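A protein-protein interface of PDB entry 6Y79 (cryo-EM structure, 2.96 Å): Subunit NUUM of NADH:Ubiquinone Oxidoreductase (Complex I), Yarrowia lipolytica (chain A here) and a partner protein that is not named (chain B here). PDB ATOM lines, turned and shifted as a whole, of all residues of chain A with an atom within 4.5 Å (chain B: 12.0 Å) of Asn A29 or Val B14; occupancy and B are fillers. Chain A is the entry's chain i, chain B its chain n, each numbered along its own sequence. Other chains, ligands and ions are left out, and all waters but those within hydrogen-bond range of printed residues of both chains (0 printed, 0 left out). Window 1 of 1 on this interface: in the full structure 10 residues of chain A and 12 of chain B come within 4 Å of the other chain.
Of the 9 printed residues of chain A, 3 touch a printed residue of chain B. Hydrophobic or aromatic side chains of chain A that line the printed part of chain B: Phe A32. Hydrophobic or aromatic side chains of chain B that line the printed part of chain A: Ala B13, Phe B16 and Phe B17.
Asn A29 touches just these residues of chain B: Val B14 (3.6 Å) and Phe B16 (3.3 Å). Printed residues of chain B within 4 Å of Asn A25: Ala B13 and Val B14. No residue of chain B comes within 4 Å of Leu A28. No residue of chain B comes within 4 Å of Gly A30. Of the printed residues of chain B, Phe A32 touches Phe B16 and Phe B17. No residue of chain B comes within 4 Å of Ala A33. Of the printed residues of chain A, Phe B17 touches Phe A32 (3.8 Å). Printed residues of chain A within 4 Å of Ala B13: Asn A25. Printed residues of chain A within 4 Å of Phe B16: Asn A29 (3.3 Å) and Phe A32 (3.7 Å). Leu B10 touches none of the printed residues of chain A. The nearest residue of chain B that does not touch Asn A29 is Pro B15 (4.6 Å). The nearest printed residue of chain A that does not touch Val B14 is Leu A28 (6.4 Å).
Asn A25 touches Ala B13 (OD1 to CB, 3.3 Å). Asn A29 touches Val B14. Phe B16 touches Asn A29. CE2 of Phe B16 touches CB of Phe A32, 3.7 Å away. Phe A32 touches Phe B17 (CE1 to CE2, 3.8 Å).
The backbone carbonyl oxygen (O) of Asn A25 is in hydrogen-bond range of the side-chain amide nitrogen (ND2) of Asn A29, at 3.0 Å.
O of Val B14 is in hydrogen-bond range of ND2 of Asn A25, 2.9 Å away.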
ATOM      1  N   ASN A  25      14.658  24.928  15.968  1.00  0.00           N
ATOM      2  CA  ASN A  25      15.844  24.079  15.952  1.00  0.00           C
ATOM      3  C   ASN A  25      16.325  23.792  17.373  1.00  0.00           C
ATOM      4  O   ASN A  25      17.455  24.088  17.744  1.00  0.00           O
ATOM      5  CB  ASN A  25      16.940  24.735  15.125  1.00  0.00           C
ATOM      6  CG  ASN A  25      17.135  26.184  15.482  1.00  0.00           C
ATOM      7  OD1 ASN A  25      16.259  26.800  16.076  1.00  0.00           O
ATOM      8  ND2 ASN A  25      18.287  26.734  15.135  1.00  0.00           N
ATOM      9  N   TRP A  26      15.463  23.175  18.174  1.00  0.00           N
ATOM     10  CA  TRP A  26      15.871  22.849  19.532  1.00  0.00           C
ATOM     11  C   TRP A  26      16.593  21.518  19.612  1.00  0.00           C
ATOM     12  O   TRP A  26      17.402  21.326  20.527  1.00  0.00           O
ATOM     13  CB  TRP A  26      14.672  22.856  20.477  1.00  0.00           C
ATOM     14  CG  TRP A  26      13.614  21.859  20.197  1.00  0.00           C
ATOM     15  CD1 TRP A  26      12.538  22.028  19.389  1.00  0.00           C
ATOM     16  CD2 TRP A  26      13.491  20.551  20.763  1.00  0.00           C
ATOM     17  NE1 TRP A  26      11.759  20.903  19.395  1.00  0.00           N
ATOM     18  CE2 TRP A  26      12.322  19.980  20.233  1.00  0.00           C
ATOM     19  CE3 TRP A  26      14.261  19.803  21.655  1.00  0.00           C
ATOM     20  CZ2 TRP A  26      11.901  18.697  20.568  1.00  0.00           C
ATOM     21  CZ3 TRP A  26      13.842  18.529  21.987  1.00  0.00           C
ATOM     22  CH2 TRP A  26      12.671  17.990  21.446  1.00  0.00           C
ATOM     23  N   LYS A  27      16.322  20.604  18.675  1.00  0.00           N
ATOM     24  CA  LYS A  27      17.181  19.439  18.482  1.00  0.00           C
ATOM     25  C   LYS A  27      18.609  19.869  18.180  1.00  0.00           C
ATOM     26  O   LYS A  27      19.546  19.476  18.886  1.00  0.00           O
ATOM     27  CB  LYS A  27      16.644  18.586  17.324  1.00  0.00           C
ATOM     28  CG  LYS A  27      15.195  18.153  17.442  1.00  0.00           C
ATOM     29  CD  LYS A  27      15.058  16.921  18.313  1.00  0.00           C
ATOM     30  CE  LYS A  27      13.629  16.418  18.349  1.00  0.00           C
ATOM     31  NZ  LYS A  27      13.187  15.942  17.016  1.00  0.00           N
ATOM     32  N   LEU A  28      18.761  20.718  17.163  1.00  0.00           N
ATOM     33  CA  LEU A  28      20.055  21.122  16.628  1.00  0.00           C
ATOM     34  C   LEU A  28      20.889  21.850  17.671  1.00  0.00           C
ATOM     35  O   LEU A  28      22.073  21.549  17.850  1.00  0.00           O
ATOM     36  CB  LEU A  28      19.817  22.005  15.408  1.00  0.00           C
ATOM     37  CG  LEU A  28      20.972  22.737  14.708  1.00  0.00           C
ATOM     38  CD1 LEU A  28      21.890  21.743  14.043  1.00  0.00           C
ATOM     39  CD2 LEU A  28      20.400  23.711  13.699  1.00  0.00           C
ATOM     40  N   ASN A  29      20.279  22.798  18.386  1.00  0.00           N
ATOM     41  CA  ASN A  29      20.969  23.460  19.485  1.00  0.00           C
ATOM     42  C   ASN A  29      21.194  22.516  20.654  1.00  0.00           C
ATOM     43  O   ASN A  29      22.150  22.696  21.424  1.00  0.00           O
ATOM     44  CB  ASN A  29      20.169  24.665  19.952  1.00  0.00           C
ATOM     45  CG  ASN A  29      20.021  25.702  18.887  1.00  0.00           C
ATOM     46  OD1 ASN A  29      20.902  25.880  18.056  1.00  0.00           O
ATOM     47  ND2 ASN A  29      18.903  26.409  18.906  1.00  0.00           N
ATOM     48  N   GLY A  30      20.313  21.524  20.820  1.00  0.00           N
ATOM     49  CA  GLY A  30      20.481  20.571  21.895  1.00  0.00           C
ATOM     50  C   GLY A  30      21.720  19.719  21.743  1.00  0.00           C
ATOM     51  O   GLY A  30      22.329  19.322  22.737  1.00  0.00           O
ATOM     52  N   LEU A  31      22.112  19.438  20.502  1.00  0.00           N
ATOM     53  CA  LEU A  31      23.370  18.728  20.262  1.00  0.00           C
ATOM     54  C   LEU A  31      24.586  19.558  20.688  1.00  0.00           C
ATOM     55  O   LEU A  31      25.551  19.016  21.251  1.00  0.00           O
ATOM     56  CB  LEU A  31      23.466  18.308  18.793  1.00  0.00           C
ATOM     57  CG  LEU A  31      22.915  16.920  18.410  1.00  0.00           C
ATOM     58  CD1 LEU A  31      21.362  16.813  18.436  1.00  0.00           C
ATOM     59  CD2 LEU A  31      23.486  16.430  17.071  1.00  0.00           C
ATOM     60  N   PHE A  32      24.540  20.882  20.465  1.00  0.00           N
ATOM     61  CA  PHE A  32      25.608  21.765  20.935  1.00  0.00           C
ATOM     62  C   PHE A  32      25.664  21.818  22.455  1.00  0.00           C
ATOM     63  O   PHE A  32      26.752  21.788  23.045  1.00  0.00           O
ATOM     64  CB  PHE A  32      25.413  23.183  20.411  1.00  0.00           C
ATOM     65  CG  PHE A  32      25.626  23.331  18.941  1.00  0.00           C
ATOM     66  CD1 PHE A  32      26.898  23.307  18.406  1.00  0.00           C
ATOM     67  CD2 PHE A  32      24.550  23.536  18.093  1.00  0.00           C
ATOM     68  CE1 PHE A  32      27.090  23.452  17.049  1.00  0.00           C
ATOM     69  CE2 PHE A  32      24.734  23.681  16.737  1.00  0.00           C
ATOM     70  CZ  PHE A  32      26.002  23.640  16.214  1.00  0.00           C
ATOM     71  N   ALA A  33      24.500  21.937  23.101  1.00  0.00           N
ATOM     72  CA  ALA A  33      24.459  21.982  24.561  1.00  0.00           C
ATOM     73  C   ALA A  33      24.927  20.667  25.171  1.00  0.00           C
ATOM     74  O   ALA A  33      25.624  20.668  26.195  1.00  0.00           O
ATOM     75  CB  ALA A  33      23.051  22.325  25.036  1.00  0.00           C
ATOM     76  N   LEU B  10       5.675  25.698  18.401  1.00  0.00           N
ATOM     77  CA  LEU B  10       7.031  26.166  18.155  1.00  0.00           C
ATOM     78  C   LEU B  10       7.081  27.692  18.106  1.00  0.00           C
ATOM     79  O   LEU B  10       6.056  28.371  18.031  1.00  0.00           O
ATOM     80  CB  LEU B  10       7.569  25.584  16.840  1.00  0.00           C
ATOM     81  CG  LEU B  10       8.125  24.157  16.726  1.00  0.00           C
ATOM     82  CD1 LEU B  10       7.053  23.083  16.848  1.00  0.00           C
ATOM     83  CD2 LEU B  10       8.848  24.003  15.405  1.00  0.00           C
ATOM     84  N   THR B  11       8.304  28.230  18.164  1.00  0.00           N
ATOM     85  CA  THR B  11       8.597  29.644  17.931  1.00  0.00           C
ATOM     86  C   THR B  11       9.720  29.670  16.888  1.00  0.00           C
ATOM     87  O   THR B  11      10.262  28.598  16.592  1.00  0.00           O
ATOM     88  CB  THR B  11       8.951  30.360  19.252  1.00  0.00           C
ATOM     89  OG1 THR B  11      10.025  29.700  19.919  1.00  0.00           O
ATOM     90  CG2 THR B  11       7.739  30.452  20.185  1.00  0.00           C
ATOM     91  N   PRO B  12      10.059  30.815  16.263  1.00  0.00           N
ATOM     92  CA  PRO B  12      11.081  30.808  15.202  1.00  0.00           C
ATOM     93  C   PRO B  12      12.471  30.357  15.636  1.00  0.00           C
ATOM     94  O   PRO B  12      12.824  30.351  16.816  1.00  0.00           O
ATOM     95  CB  PRO B  12      11.113  32.268  14.747  1.00  0.00           C
ATOM     96  CG  PRO B  12       9.738  32.703  14.912  1.00  0.00           C
ATOM     97  CD  PRO B  12       9.241  32.042  16.162  1.00  0.00           C
ATOM     98  N   ALA B  13      13.261  29.976  14.635  1.00  0.00           N
ATOM     99  CA  ALA B  13      14.586  29.428  14.873  1.00  0.00           C
ATOM    100  C   ALA B  13      15.567  30.519  15.275  1.00  0.00           C
ATOM    101  O   ALA B  13      15.504  31.651  14.788  1.00  0.00           O
ATOM    102  CB  ALA B  13      15.092  28.705  13.627  1.00  0.00           C
ATOM    103  N   VAL B  14      16.476  30.163  16.176  1.00  0.00           N
ATOM    104  CA  VAL B  14      17.479  31.061  16.742  1.00  0.00           C
ATOM    105  C   VAL B  14      18.833  30.397  16.502  1.00  0.00           C
ATOM    106  O   VAL B  14      18.941  29.173  16.658  1.00  0.00           O
ATOM    107  CB  VAL B  14      17.207  31.304  18.240  1.00  0.00           C
ATOM    108  CG1 VAL B  14      18.306  32.111  18.899  1.00  0.00           C
ATOM    109  CG2 VAL B  14      15.869  31.995  18.446  1.00  0.00           C
ATOM    110  N   PRO B  15      19.874  31.125  16.100  1.00  0.00           N
ATOM    111  CA  PRO B  15      21.199  30.510  16.017  1.00  0.00           C
ATOM    112  C   PRO B  15      21.791  30.305  17.398  1.00  0.00           C
ATOM    113  O   PRO B  15      21.548  31.079  18.324  1.00  0.00           O
ATOM    114  CB  PRO B  15      22.014  31.528  15.213  1.00  0.00           C
ATOM    115  CG  PRO B  15      21.347  32.819  15.481  1.00  0.00           C
ATOM    116  CD  PRO B  15      19.883  32.512  15.609  1.00  0.00           C
ATOM    117  N   PHE B  16      22.573  29.232  17.526  1.00  0.00           N
ATOM    118  CA  PHE B  16      23.146  28.877  18.819  1.00  0.00           C
ATOM    119  C   PHE B  16      24.205  29.882  19.247  1.00  0.00           C
ATOM    120  O   PHE B  16      24.099  30.496  20.314  1.00  0.00           O
ATOM    121  CB  PHE B  16      23.740  27.471  18.765  1.00  0.00           C
ATOM    122  CG  PHE B  16      24.373  27.038  20.050  1.00  0.00           C
ATOM    123  CD1 PHE B  16      23.586  26.683  21.130  1.00  0.00           C
ATOM    124  CD2 PHE B  16      25.752  26.991  20.183  1.00  0.00           C
ATOM    125  CE1 PHE B  16      24.155  26.289  22.317  1.00  0.00           C
ATOM    126  CE2 PHE B  16      26.329  26.601  21.374  1.00  0.00           C
ATOM    127  CZ  PHE B  16      25.525  26.249  22.441  1.00  0.00           C
ATOM    128  N   PHE B  17      25.237  30.065  18.424  1.00  0.00           N
ATOM    129  CA  PHE B  17      26.362  30.924  18.780  1.00  0.00           C
ATOM    130  C   PHE B  17      25.940  32.381  18.617  1.00  0.00           C
ATOM    131  O   PHE B  17      26.169  33.030  17.595  1.00  0.00           O
ATOM    132  CB  PHE B  17      27.586  30.578  17.950  1.00  0.00           C
ATOM    133  CG  PHE B  17      28.150  29.224  18.258  1.00  0.00           C
ATOM    134  CD1 PHE B  17      28.877  29.015  19.416  1.00  0.00           C
ATOM    135  CD2 PHE B  17      27.945  28.161  17.395  1.00  0.00           C
ATOM    136  CE1 PHE B  17      29.396  27.768  19.709  1.00  0.00           C
ATOM    137  CE2 PHE B  17      28.462  26.915  17.676  1.00  0.00           C
ATOM    138  CZ  PHE B  17      29.189  26.719  18.837  1.00  0.00           C
ATOM    139  N   GLN B  18      25.298  32.886  19.666  1.00  0.00           N
ATOM    140  CA  GLN B  18      24.985  34.294  19.809  1.00  0.00           C
ATOM    141  C   GLN B  18      26.274  35.092  20.011  1.00  0.00           C
ATOM    142  O   GLN B  18      27.313  34.517  20.344  1.00  0.00           O
ATOM    143  CB  GLN B  18      24.032  34.477  20.989  1.00  0.00           C
ATOM    144  CG  GLN B  18      22.672  33.853  20.777  1.00  0.00           C
ATOM    145  CD  GLN B  18      21.895  34.545  19.689  1.00  0.00           C
ATOM    146  OE1 GLN B  18      21.860  35.771  19.626  1.00  0.00           O
ATOM    147  NE2 GLN B  18      21.285  33.763  18.808  1.00  0.00           N
ATOM    148  N   PRO B  19      26.245  36.419  19.786  1.00  0.00           N
ATOM    149  CA  PRO B  19      27.469  37.215  19.992  1.00  0.00           C
ATOM    150  C   PRO B  19      27.980  37.221  21.418  1.00  0.00           C
ATOM    151  O   PRO B  19      29.202  37.253  21.626  1.00  0.00           O
ATOM    152  CB  PRO B  19      27.043  38.620  19.551  1.00  0.00           C
ATOM    153  CG  PRO B  19      25.997  38.384  18.562  1.00  0.00           C
ATOM    154  CD  PRO B  19      25.227  37.209  19.064  1.00  0.00           C
ATOM    155  N   TYR B  20      27.091  37.158  22.412  1.00  0.00           N
ATOM    156  CA  TYR B  20      27.568  37.115  23.787  1.00  0.00           C
ATOM    157  C   TYR B  20      28.157  35.751  24.123  1.00  0.00           C
ATOM    158  O   TYR B  20      29.132  35.669  24.869  1.00  0.00           O
ATOM    159  CB  TYR B  20      26.455  37.508  24.763  1.00  0.00           C
ATOM    160  CG  TYR B  20      25.255  36.595  24.836  1.00  0.00           C
ATOM    161  CD1 TYR B  20      24.151  36.801  24.023  1.00  0.00           C
ATOM    162  CD2 TYR B  20      25.203  35.555  25.754  1.00  0.00           C
ATOM    163  CE1 TYR B  20      23.045  35.981  24.102  1.00  0.00           C
ATOM    164  CE2 TYR B  20      24.108  34.727  25.832  1.00  0.00           C
ATOM    165  CZ  TYR B  20      23.035  34.946  25.006  1.00  0.00           C
ATOM    166  OH  TYR B  20      21.941  34.120  25.092  1.00  0.00           O
ATOM    167  N   VAL B  21      27.608  34.676  23.554  1.00  0.00           N
ATOM    168  CA  VAL B  21      28.186  33.347  23.753  1.00  0.00           C
ATOM    169  C   VAL B  21      29.613  33.303  23.227  1.00  0.00           C
ATOM    170  O   VAL B  21      30.536  32.860  23.928  1.00  0.00           O
ATOM    171  CB  VAL B  21      27.305  32.281  23.080  1.00  0.00           C
ATOM    172  CG1 VAL B  21      27.877  30.902  23.322  1.00  0.00           C
ATOM    173  CG2 VAL B  21      25.888  32.380  23.594  1.00  0.00           C
ATOM    174  N   LEU B  22      29.827  33.876  22.040  1.00  0.00           N
ATOM    175  CA  LEU B  22      31.153  33.926  21.437  1.00  0.00           C
ATOM    176  C   LEU B  22      32.104  34.786  22.256  1.00  0.00           C
ATOM    177  O   LEU B  22      33.231  34.366  22.540  1.00  0.00           O
ATOM    178  CB  LEU B  22      31.050  34.453  20.006  1.00  0.00           C
ATOM    179  CG  LEU B  22      30.267  33.565  19.044  1.00  0.00           C
ATOM    180  CD1 LEU B  22      30.007  34.283  17.733  1.00  0.00           C
ATOM    181  CD2 LEU B  22      31.019  32.269  18.820  1.00  0.00           C
